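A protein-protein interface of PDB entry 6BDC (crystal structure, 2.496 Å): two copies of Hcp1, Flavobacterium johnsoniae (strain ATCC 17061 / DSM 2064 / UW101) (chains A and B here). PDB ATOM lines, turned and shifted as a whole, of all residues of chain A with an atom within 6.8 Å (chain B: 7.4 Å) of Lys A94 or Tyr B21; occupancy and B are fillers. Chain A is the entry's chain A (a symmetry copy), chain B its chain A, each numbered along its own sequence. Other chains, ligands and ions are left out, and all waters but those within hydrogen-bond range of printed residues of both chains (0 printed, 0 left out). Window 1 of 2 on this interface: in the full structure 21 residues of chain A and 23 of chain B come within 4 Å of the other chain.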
ATOM      1  N   SER A  48      -7.716  -0.197  -2.057  1.00  0.00           N
ATOM      2  CA  SER A  48      -7.834   0.380  -3.394  1.00  0.00           C
ATOM      3  C   SER A  48      -8.004   1.894  -3.377  1.00  0.00           C
ATOM      4  O   SER A  48      -7.609   2.563  -4.339  1.00  0.00           O
ATOM      5  CB  SER A  48      -8.993  -0.273  -4.140  1.00  0.00           C
ATOM      6  OG  SER A  48      -8.636  -1.563  -4.581  1.00  0.00           O
ATOM      7  N   PHE A  55      -3.921   1.012 -11.690  1.00  0.00           N
ATOM      8  CA  PHE A  55      -4.544   0.467 -12.891  1.00  0.00           C
ATOM      9  C   PHE A  55      -3.904   1.040 -14.150  1.00  0.00           C
ATOM     10  O   PHE A  55      -3.693   0.319 -15.135  1.00  0.00           O
ATOM     11  CB  PHE A  55      -6.044   0.754 -12.867  1.00  0.00           C
ATOM     12  CG  PHE A  55      -6.789   0.232 -14.061  1.00  0.00           C
ATOM     13  CD1 PHE A  55      -7.237  -1.075 -14.097  1.00  0.00           C
ATOM     14  CD2 PHE A  55      -7.075   1.063 -15.133  1.00  0.00           C
ATOM     15  CE1 PHE A  55      -7.938  -1.551 -15.190  1.00  0.00           C
ATOM     16  CE2 PHE A  55      -7.777   0.594 -16.225  1.00  0.00           C
ATOM     17  CZ  PHE A  55      -8.205  -0.714 -16.255  1.00  0.00           C
ATOM     18  N   MET A  58      -0.609  -0.592 -15.115  1.00  0.00           N
ATOM     19  CA  MET A  58      -0.824  -1.857 -15.793  1.00  0.00           C
ATOM     20  C   MET A  58      -1.200  -1.647 -17.258  1.00  0.00           C
ATOM     21  O   MET A  58      -0.746  -2.385 -18.130  1.00  0.00           O
ATOM     22  CB  MET A  58      -1.914  -2.668 -15.092  1.00  0.00           C
ATOM     23  CG  MET A  58      -2.207  -4.001 -15.761  1.00  0.00           C
ATOM     24  SD  MET A  58      -0.796  -5.326 -15.483  1.00  0.00           S
ATOM     25  CE  MET A  58      -0.459  -5.794 -17.349  1.00  0.00           C
ATOM     26  N   LYS A  92       1.325  -8.281 -13.778  1.00  0.00           N
ATOM     27  CA  LYS A  92      -0.031  -8.753 -13.546  1.00  0.00           C
ATOM     28  C   LYS A  92      -0.727  -7.793 -12.596  1.00  0.00           C
ATOM     29  O   LYS A  92      -0.088  -7.158 -11.752  1.00  0.00           O
ATOM     30  CB  LYS A  92      -0.060 -10.175 -12.971  1.00  0.00           C
ATOM     31  N   TYR A  93      -2.049  -7.704 -12.734  1.00  0.00           N
ATOM     32  CA  TYR A  93      -2.854  -6.796 -11.931  1.00  0.00           C
ATOM     33  C   TYR A  93      -4.253  -7.374 -11.797  1.00  0.00           C
ATOM     34  O   TYR A  93      -4.771  -7.969 -12.744  1.00  0.00           O
ATOM     35  CB  TYR A  93      -2.915  -5.396 -12.558  1.00  0.00           C
ATOM     36  CG  TYR A  93      -3.829  -4.421 -11.848  1.00  0.00           C
ATOM     37  CD1 TYR A  93      -3.347  -3.609 -10.830  1.00  0.00           C
ATOM     38  CD2 TYR A  93      -5.166  -4.305 -12.201  1.00  0.00           C
ATOM     39  CE1 TYR A  93      -4.175  -2.708 -10.178  1.00  0.00           C
ATOM     40  CE2 TYR A  93      -6.003  -3.408 -11.556  1.00  0.00           C
ATOM     41  CZ  TYR A  93      -5.504  -2.612 -10.545  1.00  0.00           C
ATOM     42  OH  TYR A  93      -6.332  -1.721  -9.898  1.00  0.00           O
ATOM     43  N   LYS A  94      -4.854  -7.195 -10.622  1.00  0.00           N
ATOM     44  CA  LYS A  94      -6.223  -7.637 -10.383  1.00  0.00           C
ATOM     45  C   LYS A  94      -6.822  -6.806  -9.261  1.00  0.00           C
ATOM     46  O   LYS A  94      -6.304  -6.804  -8.141  1.00  0.00           O
ATOM     47  CB  LYS A  94      -6.274  -9.124 -10.032  1.00  0.00           C
ATOM     48  CG  LYS A  94      -7.526  -9.532  -9.272  1.00  0.00           C
ATOM     49  CD  LYS A  94      -7.628 -11.038  -9.103  1.00  0.00           C
ATOM     50  CE  LYS A  94      -8.538 -11.385  -7.936  1.00  0.00           C
ATOM     51  NZ  LYS A  94      -9.078 -12.770  -8.044  1.00  0.00           N
ATOM     52  N   GLU A  95      -7.898  -6.091  -9.568  1.00  0.00           N
ATOM     53  CA  GLU A  95      -8.693  -5.401  -8.563  1.00  0.00           C
ATOM     54  C   GLU A  95      -9.911  -6.259  -8.260  1.00  0.00           C
ATOM     55  O   GLU A  95     -10.629  -6.672  -9.175  1.00  0.00           O
ATOM     56  CB  GLU A  95      -9.112  -4.006  -9.034  1.00  0.00           C
ATOM     57  CG  GLU A  95      -9.847  -3.196  -7.969  1.00  0.00           C
ATOM     58  CD  GLU A  95      -9.731  -1.702  -8.180  1.00  0.00           C
ATOM     59  OE1 GLU A  95      -9.468  -1.279  -9.324  1.00  0.00           O
ATOM     60  OE2 GLU A  95      -9.889  -0.950  -7.198  1.00  0.00           O
ATOM     61  N   ASN A  96     -10.121  -6.548  -6.984  1.00  0.00           N
ATOM     62  CA  ASN A  96     -11.130  -7.506  -6.567  1.00  0.00           C
ATOM     63  C   ASN A  96     -11.946  -6.900  -5.442  1.00  0.00           C
ATOM     64  O   ASN A  96     -11.381  -6.369  -4.480  1.00  0.00           O
ATOM     65  CB  ASN A  96     -10.482  -8.824  -6.119  1.00  0.00           C
ATOM     66  CG  ASN A  96     -11.471  -9.778  -5.477  1.00  0.00           C
ATOM     67  OD1 ASN A  96     -12.104 -10.585  -6.157  1.00  0.00           O
ATOM     68  ND2 ASN A  96     -11.597  -9.699  -4.156  1.00  0.00           N
ATOM     69  N   PHE A  97     -13.265  -6.970  -5.571  1.00  0.00           N
ATOM     70  CA  PHE A  97     -14.170  -6.570  -4.507  1.00  0.00           C
ATOM     71  C   PHE A  97     -14.875  -7.801  -3.959  1.00  0.00           C
ATOM     72  O   PHE A  97     -15.460  -8.576  -4.720  1.00  0.00           O
ATOM     73  CB  PHE A  97     -15.198  -5.551  -4.993  1.00  0.00           C
ATOM     74  CG  PHE A  97     -16.313  -5.316  -4.013  1.00  0.00           C
ATOM     75  CD1 PHE A  97     -16.045  -4.896  -2.724  1.00  0.00           C
ATOM     76  CD2 PHE A  97     -17.627  -5.511  -4.379  1.00  0.00           C
ATOM     77  CE1 PHE A  97     -17.068  -4.679  -1.822  1.00  0.00           C
ATOM     78  CE2 PHE A  97     -18.651  -5.295  -3.472  1.00  0.00           C
ATOM     79  CZ  PHE A  97     -18.368  -4.879  -2.199  1.00  0.00           C
ATOM     80  N   THR A 106      -9.724  -4.411  -2.741  1.00  0.00           N
ATOM     81  CA  THR A 106      -8.270  -4.476  -2.705  1.00  0.00           C
ATOM     82  C   THR A 106      -7.719  -4.607  -4.118  1.00  0.00           C
ATOM     83  O   THR A 106      -8.402  -5.066  -5.039  1.00  0.00           O
ATOM     84  CB  THR A 106      -7.760  -5.657  -1.861  1.00  0.00           C
ATOM     85  OG1 THR A 106      -8.120  -6.893  -2.493  1.00  0.00           O
ATOM     86  CG2 THR A 106      -8.350  -5.617  -0.458  1.00  0.00           C
ATOM     87  N   GLU A 107      -6.457  -4.208  -4.270  1.00  0.00           N
ATOM     88  CA  GLU A 107      -5.704  -4.379  -5.505  1.00  0.00           C
ATOM     89  C   GLU A 107      -4.547  -5.336  -5.254  1.00  0.00           C
ATOM     90  O   GLU A 107      -3.775  -5.142  -4.310  1.00  0.00           O
ATOM     91  CB  GLU A 107      -5.167  -3.039  -6.012  1.00  0.00           C
ATOM     92  CG  GLU A 107      -6.197  -2.145  -6.675  1.00  0.00           C
ATOM     93  CD  GLU A 107      -5.638  -0.776  -7.013  1.00  0.00           C
ATOM     94  OE1 GLU A 107      -5.509   0.057  -6.093  1.00  0.00           O
ATOM     95  OE2 GLU A 107      -5.307  -0.540  -8.193  1.00  0.00           O
ATOM     96  N   THR A 108      -4.421  -6.354  -6.103  1.00  0.00           N
ATOM     97  CA  THR A 108      -3.359  -7.349  -5.986  1.00  0.00           C
ATOM     98  C   THR A 108      -2.607  -7.414  -7.306  1.00  0.00           C
ATOM     99  O   THR A 108      -3.199  -7.719  -8.345  1.00  0.00           O
ATOM    100  CB  THR A 108      -3.918  -8.724  -5.624  1.00  0.00           C
ATOM    101  OG1 THR A 108      -4.430  -8.694  -4.288  1.00  0.00           O
ATOM    102  CG2 THR A 108      -2.826  -9.783  -5.721  1.00  0.00           C
ATOM    103  N   PHE A 109      -1.306  -7.140  -7.267  1.00  0.00           N
ATOM    104  CA  PHE A 109      -0.531  -7.030  -8.492  1.00  0.00           C
ATOM    105  C   PHE A 109       0.873  -7.564  -8.256  1.00  0.00           C
ATOM    106  O   PHE A 109       1.325  -7.708  -7.117  1.00  0.00           O
ATOM    107  CB  PHE A 109      -0.477  -5.578  -8.994  1.00  0.00           C
ATOM    108  CG  PHE A 109       0.094  -4.607  -7.998  1.00  0.00           C
ATOM    109  CD1 PHE A 109       1.422  -4.219  -8.066  1.00  0.00           C
ATOM    110  CD2 PHE A 109      -0.699  -4.080  -6.993  1.00  0.00           C
ATOM    111  CE1 PHE A 109       1.947  -3.322  -7.149  1.00  0.00           C
ATOM    112  CE2 PHE A 109      -0.182  -3.187  -6.073  1.00  0.00           C
ATOM    113  CZ  PHE A 109       1.142  -2.807  -6.151  1.00  0.00           C
ATOM    114  N   MET A 110       1.559  -7.854  -9.357  1.00  0.00           N
ATOM    115  CA  MET A 110       2.935  -8.320  -9.303  1.00  0.00           C
ATOM    116  C   MET A 110       3.820  -7.545 -10.283  1.00  0.00           C
ATOM    117  O   MET A 110       3.505  -7.422 -11.473  1.00  0.00           O
ATOM    118  CB  MET A 110       2.997  -9.824  -9.578  1.00  0.00           C
ATOM    119  CG  MET A 110       4.166 -10.295 -10.444  1.00  0.00           C
ATOM    120  SD  MET A 110       4.484 -12.214 -10.253  1.00  0.00           S
ATOM    121  CE  MET A 110       4.974 -12.638 -12.103  1.00  0.00           C
ATOM    122  N   VAL B  19     -16.852  -8.734  -7.293  1.00  0.00           N
ATOM    123  CA  VAL B  19     -16.360  -8.385  -8.617  1.00  0.00           C
ATOM    124  C   VAL B  19     -14.862  -8.630  -8.663  1.00  0.00           C
ATOM    125  O   VAL B  19     -14.179  -8.619  -7.633  1.00  0.00           O
ATOM    126  CB  VAL B  19     -16.652  -6.920  -9.013  1.00  0.00           C
ATOM    127  CG1 VAL B  19     -17.208  -6.851 -10.432  1.00  0.00           C
ATOM    128  CG2 VAL B  19     -17.566  -6.251  -8.008  1.00  0.00           C
ATOM    129  N   SER B  20     -14.351  -8.850  -9.874  1.00  0.00           N
ATOM    130  CA  SER B  20     -12.918  -8.895 -10.117  1.00  0.00           C
ATOM    131  C   SER B  20     -12.670  -8.726 -11.610  1.00  0.00           C
ATOM    132  O   SER B  20     -13.495  -9.099 -12.446  1.00  0.00           O
ATOM    133  CB  SER B  20     -12.281 -10.197  -9.598  1.00  0.00           C
ATOM    134  OG  SER B  20     -12.250 -11.198 -10.599  1.00  0.00           O
ATOM    135  N   TYR B  21     -11.519  -8.143 -11.929  1.00  0.00           N
ATOM    136  CA  TYR B  21     -11.071  -7.979 -13.305  1.00  0.00           C
ATOM    137  C   TYR B  21      -9.556  -7.901 -13.269  1.00  0.00           C
ATOM    138  O   TYR B  21      -8.989  -7.197 -12.426  1.00  0.00           O
ATOM    139  CB  TYR B  21     -11.671  -6.726 -13.961  1.00  0.00           C
ATOM    140  CG  TYR B  21     -11.287  -5.426 -13.290  1.00  0.00           C
ATOM    141  CD1 TYR B  21     -11.981  -4.965 -12.182  1.00  0.00           C
ATOM    142  CD2 TYR B  21     -10.228  -4.661 -13.764  1.00  0.00           C
ATOM    143  CE1 TYR B  21     -11.634  -3.775 -11.561  1.00  0.00           C
ATOM    144  CE2 TYR B  21      -9.871  -3.473 -13.150  1.00  0.00           C
ATOM    145  CZ  TYR B  21     -10.580  -3.037 -12.049  1.00  0.00           C
ATOM    146  OH  TYR B  21     -10.231  -1.859 -11.431  1.00  0.00           O
ATOM    147  N   ASP B  22      -8.901  -8.636 -14.159  1.00  0.00           N
ATOM    148  CA  ASP B  22      -7.458  -8.758 -14.080  1.00  0.00           C
ATOM    149  C   ASP B  22      -6.850  -8.665 -15.470  1.00  0.00           C
ATOM    150  O   ASP B  22      -7.473  -9.034 -16.468  1.00  0.00           O
ATOM    151  CB  ASP B  22      -7.039 -10.072 -13.393  1.00  0.00           C
ATOM    152  CG  ASP B  22      -7.443 -11.297 -14.177  1.00  0.00           C
ATOM    153  OD1 ASP B  22      -6.675 -11.711 -15.070  1.00  0.00           O
ATOM    154  OD2 ASP B  22      -8.520 -11.859 -13.892  1.00  0.00           O
ATOM    155  N   LEU B  23      -5.622  -8.159 -15.512  1.00  0.00           N
ATOM    156  CA  LEU B  23      -4.837  -8.064 -16.730  1.00  0.00           C
ATOM    157  C   LEU B  23      -3.445  -8.611 -16.460  1.00  0.00           C
ATOM    158  O   LEU B  23      -2.928  -8.513 -15.343  1.00  0.00           O
ATOM    159  CB  LEU B  23      -4.723  -6.621 -17.238  1.00  0.00           C
ATOM    160  CG  LEU B  23      -5.991  -5.778 -17.375  1.00  0.00           C
ATOM    161  CD1 LEU B  23      -6.329  -5.065 -16.076  1.00  0.00           C
ATOM    162  CD2 LEU B  23      -5.829  -4.770 -18.498  1.00  0.00           C
ATOM    163  N   GLY B  40      -9.813  -7.394 -20.090  1.00  0.00           N
ATOM    164  CA  GLY B  40     -11.177  -7.165 -20.517  1.00  0.00           C
ATOM    165  C   GLY B  40     -12.180  -8.145 -19.950  1.00  0.00           C
ATOM    166  O   GLY B  40     -13.389  -7.939 -20.126  1.00  0.00           O
ATOM    167  N   ARG B  41     -11.725  -9.208 -19.287  1.00  0.00           N
ATOM    168  CA  ARG B  41     -12.616 -10.178 -18.665  1.00  0.00           C
ATOM    169  C   ARG B  41     -12.974  -9.716 -17.259  1.00  0.00           C
ATOM    170  O   ARG B  41     -12.093  -9.357 -16.472  1.00  0.00           O
ATOM    171  CB  ARG B  41     -11.966 -11.560 -18.623  1.00  0.00           C
ATOM    172  CG  ARG B  41     -12.240 -12.414 -19.855  1.00  0.00           C
ATOM    173  CD  ARG B  41     -11.220 -13.532 -20.007  1.00  0.00           C
ATOM    174  NE  ARG B  41     -11.521 -14.401 -21.143  1.00  0.00           N
ATOM    175  N   ILE B  42     -14.266  -9.723 -16.947  1.00  0.00           N
ATOM    176  CA  ILE B  42     -14.778  -9.256 -15.663  1.00  0.00           C
ATOM    177  C   ILE B  42     -15.678 -10.337 -15.077  1.00  0.00           C
ATOM    178  O   ILE B  42     -16.544 -10.877 -15.778  1.00  0.00           O
ATOM    179  CB  ILE B  42     -15.551  -7.931 -15.804  1.00  0.00           C
ATOM    180  CG1 ILE B  42     -14.719  -6.892 -16.557  1.00  0.00           C
ATOM    181  CG2 ILE B  42     -15.955  -7.405 -14.440  1.00  0.00           C
ATOM    182  CD1 ILE B  42     -15.414  -5.558 -16.710  1.00  0.00           C
ATOM    183  N   MET B  43     -15.479 -10.646 -13.797  1.00  0.00           N
ATOM    184  CA  MET B  43     -16.276 -11.658 -13.101  1.00  0.00           C
ATOM    185  C   MET B  43     -17.134 -11.012 -12.015  1.00  0.00           C
ATOM    186  O   MET B  43     -16.620 -10.265 -11.186  1.00  0.00           O
ATOM    187  CB  MET B  43     -15.373 -12.724 -12.486  1.00  0.00           C
ATOM    188  CG  MET B  43     -13.903 -12.570 -12.842  1.00  0.00           C
ATOM    189  SD  MET B  43     -13.378 -13.413 -14.518  1.00  0.00           S
ATOM    190  CE  MET B  43     -12.453 -14.975 -13.780  1.00  0.00           C
ATOM    191  N   VAL B  69     -19.415  -0.743 -13.477  1.00  0.00           N
ATOM    192  CA  VAL B  69     -19.361  -1.198 -12.093  1.00  0.00           C
ATOM    193  C   VAL B  69     -18.944  -0.008 -11.243  1.00  0.00           C
ATOM    194  O   VAL B  69     -17.855   0.546 -11.433  1.00  0.00           O
ATOM    195  CB  VAL B  69     -18.382  -2.369 -11.917  1.00  0.00           C
ATOM    196  CG1 VAL B  69     -18.303  -2.784 -10.452  1.00  0.00           C
ATOM    197  CG2 VAL B  69     -18.784  -3.543 -12.805  1.00  0.00           C
ATOM    198  N   PHE B  71     -18.206   1.518  -7.515  1.00  0.00           N
ATOM    199  CA  PHE B  71     -17.884   1.283  -6.114  1.00  0.00           C
ATOM    200  C   PHE B  71     -18.223   2.540  -5.321  1.00  0.00           C
ATOM    201  O   PHE B  71     -17.683   3.617  -5.595  1.00  0.00           O
ATOM    202  CB  PHE B  71     -16.410   0.923  -5.936  1.00  0.00           C
ATOM    203  CG  PHE B  71     -15.926  -0.146  -6.873  1.00  0.00           C
ATOM    204  CD1 PHE B  71     -15.996  -1.482  -6.517  1.00  0.00           C
ATOM    205  CD2 PHE B  71     -15.393   0.187  -8.107  1.00  0.00           C
ATOM    206  CE1 PHE B  71     -15.548  -2.466  -7.376  1.00  0.00           C
ATOM    207  CE2 PHE B  71     -14.943  -0.792  -8.971  1.00  0.00           C
ATOM    208  CZ  PHE B  71     -15.021  -2.120  -8.605  1.00  0.00           C
ATOM    209  N   LYS B  81     -15.303   5.102  -7.172  1.00  0.00           N
ATOM    210  CA  LYS B  81     -14.751   4.774  -8.476  1.00  0.00           C
ATOM    211  C   LYS B  81     -15.733   3.985  -9.302  1.00  0.00           C
ATOM    212  O   LYS B  81     -16.572   3.288  -8.759  1.00  0.00           O
ATOM    213  CB  LYS B  81     -13.450   4.000  -8.313  1.00  0.00           C
ATOM    214  N   GLU B  82     -15.635   4.105 -10.616  1.00  0.00           N
ATOM    215  CA  GLU B  82     -16.540   3.401 -11.491  1.00  0.00           C
ATOM    216  C   GLU B  82     -15.794   2.733 -12.604  1.00  0.00           C
ATOM    217  O   GLU B  82     -15.004   3.364 -13.272  1.00  0.00           O
ATOM    218  CB  GLU B  82     -17.535   4.376 -12.099  1.00  0.00           C
ATOM    219  CG  GLU B  82     -18.975   3.905 -12.128  1.00  0.00           C
ATOM    220  CD  GLU B  82     -19.869   4.829 -12.926  1.00  0.00           C
ATOM    221  OE1 GLU B  82     -19.535   5.124 -14.093  1.00  0.00           O
ATOM    222  OE2 GLU B  82     -20.902   5.261 -12.387  1.00  0.00           O
ATOM    223  N   LEU B  83     -16.086   1.468 -12.854  1.00  0.00           N
ATOM    224  CA  LEU B  83     -15.430   0.777 -13.938  1.00  0.00           C
ATOM    225  C   LEU B  83     -16.406   0.651 -15.061  1.00  0.00           C
ATOM    226  O   LEU B  83     -17.494   0.137 -14.886  1.00  0.00           O
ATOM    227  CB  LEU B  83     -15.000  -0.609 -13.502  1.00  0.00           C
ATOM    228  CG  LEU B  83     -13.971  -1.287 -14.397  1.00  0.00           C
ATOM    229  CD1 LEU B  83     -14.040  -2.786 -14.223  1.00  0.00           C
ATOM    230  CD2 LEU B  83     -14.153  -0.913 -15.853  1.00  0.00           C
ATOM    231  N   ILE B 116     -12.190  -1.874 -21.416  1.00  0.00           N
ATOM    232  CA  ILE B 116     -12.491  -1.394 -20.075  1.00  0.00           C
ATOM    233  C   ILE B 116     -11.719  -0.099 -19.864  1.00  0.00           C
ATOM    234  O   ILE B 116     -10.668   0.133 -20.469  1.00  0.00           O
ATOM    235  CB  ILE B 116     -12.140  -2.420 -18.979  1.00  0.00           C
ATOM    236  CG1 ILE B 116     -10.674  -2.850 -19.095  1.00  0.00           C
ATOM    237  CG2 ILE B 116     -13.063  -3.627 -19.059  1.00  0.00           C
ATOM    238  CD1 ILE B 116     -10.231  -3.842 -18.029  1.00  0.00           C
ATOM    239  N   SER B 117     -12.256   0.753 -18.994  1.00  0.00           N
ATOM    240  CA  SER B 117     -11.637   2.042 -18.724  1.00  0.00           C
ATOM    241  C   SER B 117     -11.971   2.471 -17.305  1.00  0.00           C
ATOM    242  O   SER B 117     -13.040   2.145 -16.779  1.00  0.00           O
ATOM    243  CB  SER B 117     -12.103   3.111 -19.718  1.00  0.00           C
ATOM    244  OG  SER B 117     -13.356   3.639 -19.323  1.00  0.00           O
ATOM    245  N   MET B 118     -11.051   3.220 -16.700  1.00  0.00           N
ATOM    246  CA  MET B 118     -11.216   3.677 -15.323  1.00  0.00           C
ATOM    247  C   MET B 118     -10.183   4.743 -14.949  1.00  0.00           C
ATOM    248  O   MET B 118      -8.974   4.516 -15.069  1.00  0.00           O
ATOM    249  CB  MET B 118     -11.126   2.479 -14.369  1.00  0.00           C
ATOM    250  CG  MET B 118     -11.426   2.783 -12.916  1.00  0.00           C
ATOM    251  SD  MET B 118     -11.828   1.149 -11.948  1.00  0.00           S
ATOM    252  CE  MET B 118     -11.550   1.767 -10.128  1.00  0.00           C
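Among the printed residues, merely in contact across the chains: Tyr A93 with Asp B22, Glu A95 with Ser B20, Phe A55 with Tyr B21, Lys A92 with Leu B23, Lys A94 with Tyr B21, Asn A96 with Ser B20, Lys A94 with Asp B22, Glu A95 with Met B118, Met A58 with Leu B23, Phe A97 with Phe B71, Phe A55 with Met B118 and Phe A55 with Leu B23.
The backbone carbonyl oxygen of Ser B20 sits at hydrogen-bond distance from the backbone NH of Met B43 (2.9 Å).
The side-chain hydroxyl of Tyr B21 lies within hydrogen-bond range of the side-chain sulfur of Met B118.
The backbone carbonyl oxygen (O) of Lys B81 lies within hydrogen-bond range of the backbone NH (N) of Phe B71 (2.7 Å).
OG of Ser A48 lies within hydrogen-bond range of OE2 of Glu A95, 3.0 Å away.
O of Lys A94 lies within hydrogen-bond range of N of Thr A108 (2.8 Å).
N of Asn A96 lies within hydrogen-bond range of O of Thr A106, 3.0 Å away.
Of chain B, only Tyr B21 and Asp B22 come within 4 Å of Lys A94.
Of chain A, only Phe A55 (3.4 Å), Lys A94 (3.5 Å) and Glu A95 (2.3 Å) come within 4 Å of Tyr B21.
Of the printed residues of chain A, Met B118 touches Phe A55 and Glu A95.
Printed residues of chain B within 4 Å of Lys A92: Leu B23.
The nearest residue of chain B that does not touch Lys A94 is Ser B20 (4.3 Å).
No position is printed for both chains.
Of the 16 pairs that touch across the chains among the printed residues, none has its exchanged pair printed and touching as well.
Of the 17 printed residues of chain B, 7 touch a printed residue of chain A.
Hydrophobic or aromatic side chains of chain B within 4 Å of the printed part of chain A: Val B19, Tyr B21, Leu B23, Phe B71 and Met B118.
Hydrophobic or aromatic side chains of chain A that line the printed part of chain B: Phe A55, Met A58 and Phe A97.
Along chain A the printed residues that touch a printed residue of chain B span positions 55 to 97.
Among the printed residues, no Asp or Glu carboxylate lies within 4 Å of a Lys or Arg side-chain nitrogen of the other chain.
O of Val B19 lies close to OD1 of Asn A96.
The backbone carbonyl oxygen (O) of Val B19 lies within hydrogen-bond range of the backbone NH (N) of Phe A97 (2.8 Å).
The backbone NH of Tyr B21 lies within hydrogen-bond range of the backbone carbonyl oxygen of Glu A95, 3.2 Å away.
O of Leu B23 lies within hydrogen-bond range of N of Tyr A93, at 2.9 Å.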
